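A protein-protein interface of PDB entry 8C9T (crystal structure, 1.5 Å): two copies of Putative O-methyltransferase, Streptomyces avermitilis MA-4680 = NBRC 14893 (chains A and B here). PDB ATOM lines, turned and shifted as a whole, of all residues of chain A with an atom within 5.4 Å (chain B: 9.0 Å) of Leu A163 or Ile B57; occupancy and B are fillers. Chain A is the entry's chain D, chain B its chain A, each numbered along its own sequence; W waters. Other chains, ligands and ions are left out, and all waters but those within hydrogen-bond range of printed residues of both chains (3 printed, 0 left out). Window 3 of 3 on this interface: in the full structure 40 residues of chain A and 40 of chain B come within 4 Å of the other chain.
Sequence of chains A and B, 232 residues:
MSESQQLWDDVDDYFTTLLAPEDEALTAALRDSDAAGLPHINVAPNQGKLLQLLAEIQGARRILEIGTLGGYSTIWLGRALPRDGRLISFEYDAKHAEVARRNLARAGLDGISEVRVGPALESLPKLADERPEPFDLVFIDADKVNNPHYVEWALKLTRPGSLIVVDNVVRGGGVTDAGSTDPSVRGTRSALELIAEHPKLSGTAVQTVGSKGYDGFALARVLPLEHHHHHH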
ATOM      1  N   LEU A  54      -2.715  26.298 -20.165  1.00  0.00           N
ATOM      2  CA  LEU A  54      -2.326  26.867 -18.847  1.00  0.00           C
ATOM      3  C   LEU A  54      -3.033  26.080 -17.732  1.00  0.00           C
ATOM      4  O   LEU A  54      -2.397  25.666 -16.761  1.00  0.00           O
ATOM      5  CB  LEU A  54      -2.654  28.363 -18.755  1.00  0.00           C
ATOM      6  CG  LEU A  54      -1.823  29.333 -19.593  1.00  0.00           C
ATOM      7  CD1 LEU A  54      -2.404  30.742 -19.629  1.00  0.00           C
ATOM      8  CD2 LEU A  54      -0.380  29.405 -19.064  1.00  0.00           C
ATOM      9  N   ILE A  57      -1.472  22.553 -17.470  1.00  0.00           N
ATOM     10  CA  ILE A  57      -0.118  22.600 -16.851  1.00  0.00           C
ATOM     11  C   ILE A  57      -0.260  22.837 -15.350  1.00  0.00           C
ATOM     12  O   ILE A  57       0.527  22.258 -14.557  1.00  0.00           O
ATOM     13  CB  ILE A  57       0.733  23.677 -17.526  1.00  0.00           C
ATOM     14  CG1 ILE A  57       0.931  23.390 -19.018  1.00  0.00           C
ATOM     15  CG2 ILE A  57       2.053  23.848 -16.814  1.00  0.00           C
ATOM     16  CD1 ILE A  57       1.225  24.619 -19.802  1.00  0.00           C
ATOM     17  N   GLN A  58      -1.231  23.644 -14.939  1.00  0.00           N
ATOM     18  CA  GLN A  58      -1.447  23.913 -13.499  1.00  0.00           C
ATOM     19  C   GLN A  58      -1.983  22.681 -12.787  1.00  0.00           C
ATOM     20  O   GLN A  58      -1.858  22.597 -11.572  1.00  0.00           O
ATOM     21  CB  GLN A  58      -2.420  25.077 -13.364  1.00  0.00           C
ATOM     22  CG  GLN A  58      -2.450  25.691 -11.969  1.00  0.00           C
ATOM     23  CD  GLN A  58      -3.306  25.028 -10.947  1.00  0.00           C
ATOM     24  OE1 GLN A  58      -4.270  24.315 -11.254  1.00  0.00           O
ATOM     25  NE2 GLN A  58      -2.984  25.359  -9.699  1.00  0.00           N
ATOM     26  N   ASP A 136      -8.703  26.232  -8.412  1.00  0.00           N
ATOM     27  CA  ASP A 136      -7.311  26.097  -8.888  1.00  0.00           C
ATOM     28  C   ASP A 136      -6.940  27.176  -9.877  1.00  0.00           C
ATOM     29  O   ASP A 136      -5.764  27.579  -9.937  1.00  0.00           O
ATOM     30  CB  ASP A 136      -7.057  24.736  -9.523  1.00  0.00           C
ATOM     31  CG  ASP A 136      -7.295  23.637  -8.532  1.00  0.00           C
ATOM     32  OD1 ASP A 136      -6.769  23.763  -7.430  1.00  0.00           O
ATOM     33  OD2 ASP A 136      -8.070  22.692  -8.885  1.00  0.00           O
ATOM     34  N   LEU A 137      -7.897  27.643 -10.690  1.00  0.00           N
ATOM     35  CA  LEU A 137      -7.648  28.688 -11.688  1.00  0.00           C
ATOM     36  C   LEU A 137      -8.880  29.577 -11.763  1.00  0.00           C
ATOM     37  O   LEU A 137     -10.015  29.074 -11.766  1.00  0.00           O
ATOM     38  CB  LEU A 137      -7.298  28.068 -13.042  1.00  0.00           C
ATOM     39  CG  LEU A 137      -6.880  29.055 -14.114  1.00  0.00           C
ATOM     40  CD1 LEU A 137      -5.925  28.395 -15.111  1.00  0.00           C
ATOM     41  CD2 LEU A 137      -8.100  29.633 -14.804  1.00  0.00           C
ATOM     42  N   VAL A 138      -8.655  30.873 -11.682  1.00  0.00           N
ATOM     43  CA  VAL A 138      -9.727  31.869 -11.907  1.00  0.00           C
ATOM     44  C   VAL A 138      -9.375  32.652 -13.149  1.00  0.00           C
ATOM     45  O   VAL A 138      -8.239  33.189 -13.228  1.00  0.00           O
ATOM     46  CB  VAL A 138      -9.880  32.812 -10.715  1.00  0.00           C
ATOM     47  CG1 VAL A 138     -11.016  33.812 -10.958  1.00  0.00           C
ATOM     48  CG2 VAL A 138     -10.084  32.042  -9.433  1.00  0.00           C
ATOM     49  N   THR A 158      -9.322  31.110  -3.853  1.00  0.00           N
ATOM     50  CA  THR A 158      -8.197  30.261  -4.298  1.00  0.00           C
ATOM     51  C   THR A 158      -7.408  29.745  -3.093  1.00  0.00           C
ATOM     52  O   THR A 158      -7.787  30.025  -1.917  1.00  0.00           O
ATOM     53  CB  THR A 158      -7.347  31.038  -5.322  1.00  0.00           C
ATOM     54  OG1 THR A 158      -6.965  32.321  -4.819  1.00  0.00           O
ATOM     55  CG2 THR A 158      -8.054  31.196  -6.648  1.00  0.00           C
ATOM     56  N   GLY A 161      -0.788  28.146  -4.756  1.00  0.00           N
ATOM     57  CA  GLY A 161      -0.512  27.429  -6.009  1.00  0.00           C
ATOM     58  C   GLY A 161      -1.546  27.618  -7.082  1.00  0.00           C
ATOM     59  O   GLY A 161      -1.261  27.286  -8.224  1.00  0.00           O
ATOM     60  N   SER A 162      -2.688  28.190  -6.716  1.00  0.00           N
ATOM     61  CA  SER A 162      -3.698  28.570  -7.727  1.00  0.00           C
ATOM     62  C   SER A 162      -3.149  29.601  -8.704  1.00  0.00           C
ATOM     63  O   SER A 162      -2.161  30.301  -8.406  1.00  0.00           O
ATOM     64  CB  SER A 162      -4.949  29.122  -7.084  1.00  0.00           C
ATOM     65  OG  SER A 162      -5.641  28.144  -6.319  1.00  0.00           O
ATOM     66  N   LEU A 163      -3.803  29.739  -9.841  1.00  0.00           N
ATOM     67  CA  LEU A 163      -3.440  30.676 -10.910  1.00  0.00           C
ATOM     68  C   LEU A 163      -4.622  31.599 -11.156  1.00  0.00           C
ATOM     69  O   LEU A 163      -5.786  31.138 -11.135  1.00  0.00           O
ATOM     70  CB  LEU A 163      -3.079  29.892 -12.171  1.00  0.00           C
ATOM     71  CG  LEU A 163      -2.504  30.644 -13.382  1.00  0.00           C
ATOM     72  CD1 LEU A 163      -1.212  31.376 -13.033  1.00  0.00           C
ATOM     73  CD2 LEU A 163      -2.286  29.709 -14.578  1.00  0.00           C
ATOM     74  N   ILE A 164      -4.353  32.861 -11.337  1.00  0.00           N
ATOM     75  CA  ILE A 164      -5.342  33.882 -11.755  1.00  0.00           C
ATOM     76  C   ILE A 164      -4.911  34.382 -13.122  1.00  0.00           C
ATOM     77  O   ILE A 164      -3.745  34.775 -13.279  1.00  0.00           O
ATOM     78  CB  ILE A 164      -5.455  35.025 -10.744  1.00  0.00           C
ATOM     79  CG1 ILE A 164      -5.799  34.488  -9.358  1.00  0.00           C
ATOM     80  CG2 ILE A 164      -6.409  36.088 -11.247  1.00  0.00           C
ATOM     81  CD1 ILE A 164      -5.615  35.489  -8.226  1.00  0.00           C
ATOM     82  N   VAL A 165      -5.815  34.386 -14.074  1.00  0.00           N
ATOM     83  CA  VAL A 165      -5.541  34.862 -15.450  1.00  0.00           C
ATOM     84  C   VAL A 165      -6.492  36.003 -15.735  1.00  0.00           C
ATOM     85  O   VAL A 165      -7.700  35.851 -15.503  1.00  0.00           O
ATOM     86  CB  VAL A 165      -5.684  33.740 -16.480  1.00  0.00           C
ATOM     87  CG1 VAL A 165      -5.456  34.305 -17.887  1.00  0.00           C
ATOM     88  CG2 VAL A 165      -4.797  32.553 -16.110  1.00  0.00           C
ATOM     89  N   LEU A 219      -0.988  37.058 -15.986  1.00  0.00           N
ATOM     90  CA  LEU A 219      -0.993  35.791 -15.224  1.00  0.00           C
ATOM     91  C   LEU A 219      -0.534  36.128 -13.835  1.00  0.00           C
ATOM     92  O   LEU A 219       0.460  36.864 -13.706  1.00  0.00           O
ATOM     93  CB  LEU A 219       0.026  34.796 -15.792  1.00  0.00           C
ATOM     94  CG  LEU A 219      -0.165  34.246 -17.171  1.00  0.00           C
ATOM     95  CD1 LEU A 219       0.787  33.052 -17.364  1.00  0.00           C
ATOM     96  CD2 LEU A 219      -1.594  33.793 -17.353  1.00  0.00           C
ATOM     97  N   ALA A 220      -1.108  35.527 -12.816  1.00  0.00           N
ATOM     98  CA  ALA A 220      -0.606  35.711 -11.445  1.00  0.00           C
ATOM     99  C   ALA A 220      -0.720  34.393 -10.716  1.00  0.00           C
ATOM    100  O   ALA A 220      -1.788  33.766 -10.730  1.00  0.00           O
ATOM    101  CB  ALA A 220      -1.334  36.780 -10.745  1.00  0.00           C
ATOM    102  N   ARG A 221       0.351  33.958 -10.083  1.00  0.00           N
ATOM    103  CA  ARG A 221       0.364  32.721  -9.295  1.00  0.00           C
ATOM    104  C   ARG A 221       0.203  33.100  -7.838  1.00  0.00           C
ATOM    105  O   ARG A 221       0.831  34.039  -7.392  1.00  0.00           O
ATOM    106  CB  ARG A 221       1.691  32.024  -9.524  1.00  0.00           C
ATOM    107  CG  ARG A 221       1.809  30.698  -8.844  1.00  0.00           C
ATOM    108  CD  ARG A 221       2.890  29.935  -9.620  1.00  0.00           C
ATOM    109  NE  ARG A 221       2.951  28.627  -9.027  1.00  0.00           N
ATOM    110  CZ  ARG A 221       3.843  28.274  -8.152  1.00  0.00           C
ATOM    111  NH1 ARG A 221       3.793  27.059  -7.636  1.00  0.00           N
ATOM    112  NH2 ARG A 221       4.789  29.120  -7.796  1.00  0.00           N
ATOM    113  N   VAL A 222      -0.653  32.372  -7.148  1.00  0.00           N
ATOM    114  CA  VAL A 222      -0.831  32.510  -5.684  1.00  0.00           C
ATOM    115  C   VAL A 222       0.305  31.738  -4.986  1.00  0.00           C
ATOM    116  O   VAL A 222       0.496  30.535  -5.278  1.00  0.00           O
ATOM    117  CB  VAL A 222      -2.214  32.023  -5.246  1.00  0.00           C
ATOM    118  CG1 VAL A 222      -2.351  32.170  -3.737  1.00  0.00           C
ATOM    119  CG2 VAL A 222      -3.353  32.730  -5.966  1.00  0.00           C
ATOM    120  N   LYS B  49       9.661  36.605 -17.422  1.00  0.00           N
ATOM    121  CA  LYS B  49       8.900  36.193 -16.235  1.00  0.00           C
ATOM    122  C   LYS B  49       7.790  35.225 -16.634  1.00  0.00           C
ATOM    123  O   LYS B  49       7.422  34.395 -15.828  1.00  0.00           O
ATOM    124  CB  LYS B  49       8.395  37.405 -15.465  1.00  0.00           C
ATOM    125  CG  LYS B  49       7.828  36.983 -14.136  1.00  0.00           C
ATOM    126  CD  LYS B  49       7.811  37.979 -13.067  1.00  0.00           C
ATOM    127  CE  LYS B  49       7.237  37.325 -11.836  1.00  0.00           C
ATOM    128  NZ  LYS B  49       6.643  38.355 -10.996  1.00  0.00           N
ATOM    129  N   LEU B  50       7.200  35.417 -17.803  1.00  0.00           N
ATOM    130  CA  LEU B  50       6.194  34.437 -18.297  1.00  0.00           C
ATOM    131  C   LEU B  50       6.851  33.055 -18.408  1.00  0.00           C
ATOM    132  O   LEU B  50       6.250  32.114 -17.929  1.00  0.00           O
ATOM    133  CB  LEU B  50       5.627  34.895 -19.636  1.00  0.00           C
ATOM    134  CG  LEU B  50       4.633  33.914 -20.252  1.00  0.00           C
ATOM    135  CD1 LEU B  50       3.467  33.740 -19.330  1.00  0.00           C
ATOM    136  CD2 LEU B  50       4.179  34.409 -21.625  1.00  0.00           C
ATOM    137  N   LEU B  51       8.074  32.955 -18.917  1.00  0.00           N
ATOM    138  CA  LEU B  51       8.801  31.633 -18.986  1.00  0.00           C
ATOM    139  C   LEU B  51       9.014  31.067 -17.585  1.00  0.00           C
ATOM    140  O   LEU B  51       8.761  29.917 -17.328  1.00  0.00           O
ATOM    141  CB  LEU B  51      10.156  31.821 -19.669  1.00  0.00           C
ATOM    142  CG  LEU B  51      10.220  31.987 -21.178  1.00  0.00           C
ATOM    143  CD1 LEU B  51      11.680  32.122 -21.578  1.00  0.00           C
ATOM    144  CD2 LEU B  51       9.590  30.776 -21.860  1.00  0.00           C
ATOM    145  N   GLN B  52       9.422  31.925 -16.643  1.00  0.00           N
ATOM    146  CA  GLN B  52       9.657  31.507 -15.245  1.00  0.00           C
ATOM    147  C   GLN B  52       8.347  30.959 -14.679  1.00  0.00           C
ATOM    148  O   GLN B  52       8.326  29.923 -14.061  1.00  0.00           O
ATOM    149  CB  GLN B  52      10.230  32.700 -14.457  1.00  0.00           C
ATOM    150  CG  GLN B  52      10.492  32.350 -12.986  1.00  0.00           C
ATOM    151  CD  GLN B  52      10.733  33.484 -12.013  1.00  0.00           C
ATOM    152  OE1 GLN B  52      10.659  33.281 -10.791  1.00  0.00           O
ATOM    153  NE2 GLN B  52      11.095  34.648 -12.463  1.00  0.00           N
ATOM    154  N   LEU B  53       7.254  31.690 -14.868  1.00  0.00           N
ATOM    155  CA  LEU B  53       5.969  31.318 -14.256  1.00  0.00           C
ATOM    156  C   LEU B  53       5.464  30.033 -14.908  1.00  0.00           C
ATOM    157  O   LEU B  53       4.989  29.184 -14.168  1.00  0.00           O
ATOM    158  CB  LEU B  53       4.990  32.476 -14.474  1.00  0.00           C
ATOM    159  CG  LEU B  53       5.175  33.625 -13.496  1.00  0.00           C
ATOM    160  CD1 LEU B  53       4.408  34.834 -13.992  1.00  0.00           C
ATOM    161  CD2 LEU B  53       4.734  33.239 -12.090  1.00  0.00           C
ATOM    162  N   LEU B  54       5.651  29.883 -16.220  1.00  0.00           N
ATOM    163  CA  LEU B  54       5.224  28.620 -16.893  1.00  0.00           C
ATOM    164  C   LEU B  54       5.953  27.457 -16.202  1.00  0.00           C
ATOM    165  O   LEU B  54       5.343  26.438 -15.868  1.00  0.00           O
ATOM    166  CB  LEU B  54       5.559  28.623 -18.395  1.00  0.00           C
ATOM    167  CG  LEU B  54       4.714  29.508 -19.322  1.00  0.00           C
ATOM    168  CD1 LEU B  54       5.283  29.618 -20.743  1.00  0.00           C
ATOM    169  CD2 LEU B  54       3.261  29.060 -19.338  1.00  0.00           C
ATOM    170  N   ALA B  55       7.261  27.586 -15.966  1.00  0.00           N
ATOM    171  CA  ALA B  55       8.025  26.517 -15.301  1.00  0.00           C
ATOM    172  C   ALA B  55       7.485  26.287 -13.890  1.00  0.00           C
ATOM    173  O   ALA B  55       7.289  25.164 -13.476  1.00  0.00           O
ATOM    174  CB  ALA B  55       9.485  26.903 -15.278  1.00  0.00           C
ATOM    175  N   GLU B  56       7.214  27.350 -13.151  1.00  0.00           N
ATOM    176  CA  GLU B  56       6.760  27.184 -11.744  1.00  0.00           C
ATOM    177  C   GLU B  56       5.360  26.586 -11.685  1.00  0.00           C
ATOM    178  O   GLU B  56       5.150  25.735 -10.861  1.00  0.00           O
ATOM    179  CB  GLU B  56       6.763  28.538 -11.045  1.00  0.00           C
ATOM    180  CG  GLU B  56       8.163  29.098 -10.816  1.00  0.00           C
ATOM    181  CD  GLU B  56       8.171  30.497 -10.213  1.00  0.00           C
ATOM    182  OE1 GLU B  56       7.170  31.213 -10.345  1.00  0.00           O
ATOM    183  OE2 GLU B  56       9.210  30.898  -9.731  1.00  0.00           O
ATOM    184  N   ILE B  57       4.499  27.003 -12.582  1.00  0.00           N
ATOM    185  CA  ILE B  57       3.105  26.473 -12.701  1.00  0.00           C
ATOM    186  C   ILE B  57       3.219  24.968 -12.989  1.00  0.00           C
ATOM    187  O   ILE B  57       2.474  24.158 -12.416  1.00  0.00           O
ATOM    188  CB  ILE B  57       2.301  27.241 -13.755  1.00  0.00           C
ATOM    189  CG1 ILE B  57       2.057  28.710 -13.363  1.00  0.00           C
ATOM    190  CG2 ILE B  57       0.991  26.494 -13.981  1.00  0.00           C
ATOM    191  CD1 ILE B  57       1.674  29.612 -14.459  1.00  0.00           C
ATOM    192  N   GLN B  58       4.083  24.585 -13.925  1.00  0.00           N
ATOM    193  CA  GLN B  58       4.227  23.168 -14.316  1.00  0.00           C
ATOM    194  C   GLN B  58       4.784  22.316 -13.179  1.00  0.00           C
ATOM    195  O   GLN B  58       4.558  21.077 -13.188  1.00  0.00           O
ATOM    196  CB  GLN B  58       5.162  23.125 -15.521  1.00  0.00           C
ATOM    197  CG  GLN B  58       5.197  21.774 -16.243  1.00  0.00           C
ATOM    198  CD  GLN B  58       6.184  20.782 -15.699  1.00  0.00           C
ATOM    199  OE1 GLN B  58       7.136  21.105 -14.964  1.00  0.00           O
ATOM    200  NE2 GLN B  58       5.990  19.515 -16.079  1.00  0.00           N
ATOM    201  N   GLY B  59       5.540  22.904 -12.253  1.00  0.00           N
ATOM    202  CA  GLY B  59       6.249  22.244 -11.160  1.00  0.00           C
ATOM    203  C   GLY B  59       7.624  21.762 -11.579  1.00  0.00           C
ATOM    204  O   GLY B  59       8.112  20.784 -11.062  1.00  0.00           O
ATOM    205  N   ALA B  60       8.269  22.504 -12.473  1.00  0.00           N
ATOM    206  CA  ALA B  60       9.489  22.008 -13.123  1.00  0.00           C
ATOM    207  C   ALA B  60      10.622  21.848 -12.111  1.00  0.00           C
ATOM    208  O   ALA B  60      10.820  22.753 -11.282  1.00  0.00           O
ATOM    209  CB  ALA B  60       9.934  22.949 -14.210  1.00  0.00           C
ATOM    210  N   ALA B  80      13.037  29.660 -11.615  1.00  0.00           N
ATOM    211  CA  ALA B  80      11.859  28.813 -11.337  1.00  0.00           C
ATOM    212  C   ALA B  80      12.212  27.583 -10.511  1.00  0.00           C
ATOM    213  O   ALA B  80      11.280  26.963 -10.009  1.00  0.00           O
ATOM    214  CB  ALA B  80      11.255  28.358 -12.624  1.00  0.00           C
ATOM    215  N   LEU B 137      10.698  20.837 -18.664  1.00  0.00           N
ATOM    216  CA  LEU B 137      10.456  21.943 -19.624  1.00  0.00           C
ATOM    217  C   LEU B 137      11.660  21.980 -20.554  1.00  0.00           C
ATOM    218  O   LEU B 137      12.804  21.972 -20.078  1.00  0.00           O
ATOM    219  CB  LEU B 137      10.212  23.267 -18.913  1.00  0.00           C
ATOM    220  CG  LEU B 137       9.766  24.436 -19.796  1.00  0.00           C
ATOM    221  CD1 LEU B 137       8.898  25.464 -18.992  1.00  0.00           C
ATOM    222  CD2 LEU B 137      10.946  25.119 -20.418  1.00  0.00           C
ATOM    223  N   GLY B 161       3.380  15.183 -19.343  1.00  0.00           N
ATOM    224  CA  GLY B 161       3.231  16.403 -18.555  1.00  0.00           C
ATOM    225  C   GLY B 161       4.349  17.406 -18.739  1.00  0.00           C
ATOM    226  O   GLY B 161       4.194  18.551 -18.295  1.00  0.00           O
ATOM    227  N   LEU B 163       6.588  20.181 -20.682  1.00  0.00           N
ATOM    228  CA  LEU B 163       6.222  21.327 -21.556  1.00  0.00           C
ATOM    229  C   LEU B 163       7.399  21.638 -22.505  1.00  0.00           C
ATOM    230  O   LEU B 163       8.558  21.747 -21.999  1.00  0.00           O
ATOM    231  CB  LEU B 163       5.848  22.525 -20.663  1.00  0.00           C
ATOM    232  CG  LEU B 163       5.232  23.736 -21.375  1.00  0.00           C
ATOM    233  CD1 LEU B 163       3.886  23.342 -21.941  1.00  0.00           C
ATOM    234  CD2 LEU B 163       5.132  24.987 -20.476  1.00  0.00           C
ATOM    235  N   ARG B 221       2.336  20.654 -24.643  1.00  0.00           N
ATOM    236  CA  ARG B 221       2.341  19.715 -23.535  1.00  0.00           C
ATOM    237  C   ARG B 221       2.527  18.285 -24.057  1.00  0.00           C
ATOM    238  O   ARG B 221       1.880  17.906 -25.024  1.00  0.00           O
ATOM    239  CB  ARG B 221       1.055  19.911 -22.748  1.00  0.00           C
ATOM    240  CG  ARG B 221       1.067  19.219 -21.413  1.00  0.00           C
ATOM    241  CD  ARG B 221      -0.067  19.821 -20.579  1.00  0.00           C
ATOM    242  NE  ARG B 221      -0.118  19.118 -19.338  1.00  0.00           N
ATOM    243  CZ  ARG B 221      -0.898  18.091 -19.089  1.00  0.00           C
ATOM    244  NH1 ARG B 221      -1.814  17.735 -19.974  1.00  0.00           N
ATOM    245  NH2 ARG B 221      -0.799  17.477 -17.928  1.00  0.00           N
HETATM  246  O   HOH W   1       5.435  31.837  -8.356  1.00  0.00           O
HETATM  247  O   HOH W   2       2.410  19.975 -15.041  1.00  0.00           O
HETATM  248  O   HOH W   3       0.661  24.549 -10.308  1.00  0.00           O
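The backbone carbonyl oxygen (O) of Ile A57 lies close to the backbone carbonyl oxygen (O) of Ile B57 (3.5 Å).
Water W1 bridges the side-chain carboxylate (OE1) of Glu B56 and the guanidinium group (NH2) of Arg A221.
Water W3 bridges O of Ile B57 (2.8 Å) and O of Gln A58 (3.4 Å).
Water W2 lies within hydrogen-bond range of O of Ile A57 (3.0 Å) and O of Gln B58 (3.0 Å).
Of the 17 printed residues of chain B, 6 touch a printed residue of chain A.
Hydrophobic or aromatic side chains of chain B within 4 Å of the printed part of chain A: Leu B50, Leu B54, Ile B57 and Leu B163.
Printed residues of chain A that touch a printed residue of chain B: Leu A54, Ile A57, Gln A58, Leu A163, Leu A219 and Arg A221.
Among the printed residues, 8 pairs touch across the chains.
Among the printed residues, no Asp or Glu carboxylate lies within 4 Å of a Lys or Arg side-chain nitrogen of the other chain.
Of chain A, only Ile A57, Gln A58 and Leu A163 come within 4 Å of Ile B57.
No residue of chain B comes within 4 Å of Leu A137.
No residue of chain B comes within 4 Å of Ser A162.
Printed residues of chain B within 4 Å of Leu A54: Leu B54.
Printed residues of chain B within 4 Å of Leu A219: Leu B50.
Of the printed residues of chain A, Leu B54 touches Leu A54.
The nearest residue of chain A that does not touch Ile B57 is Arg A221 (4.03 Å).
Leu A54 touches Leu B54 (CD2 to CD2, 3.7 Å).
Gln B58 touches Ile A57.
Ile A57 touches Leu B163.
Gln A58 touches Ile B57 (CA to CG2, 3.6 Å).
Ile B57 touches Leu A163.
Leu A219 touches Leu B50.
Arg A221 touches Glu B56 (NH1 to O, 3.7 Å).
Leu A54 touches its own counterpart, Leu B54.
Ile B57 touches its own counterpart, Ile A57.
Ile A57 touches Gln B58, and with the chains exchanged Gln A58 touches Ile B57.
Ile A57 touches Leu B163, and with the chains exchanged Leu A163 touches Ile B57.
7 positions are printed for both chains.
The backbone carbonyl oxygen of Asp A136 lies within hydrogen-bond range of the backbone NH of Leu A163 (2.9 Å).
The side-chain carboxylate (OE2) of Glu B56 lies close to the side-chain amide oxygen (OE1) of Gln B52, 3.0 Å away.
NE2 of Gln B58 is in hydrogen-bond range of O of Gly B161 (3.0 Å).
The backbone carbonyl oxygen (O) of Gly A161 sits at hydrogen-bond distance from the side-chain amide nitrogen (NE2) of Gln A58 (3.0 Å).
The side-chain amide oxygen of Gln B58 is in hydrogen-bond range of the backbone NH of Ala B60 (3.1 Å).
N of Val A138 sits at hydrogen-bond distance from O of Leu A163 (2.9 Å).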
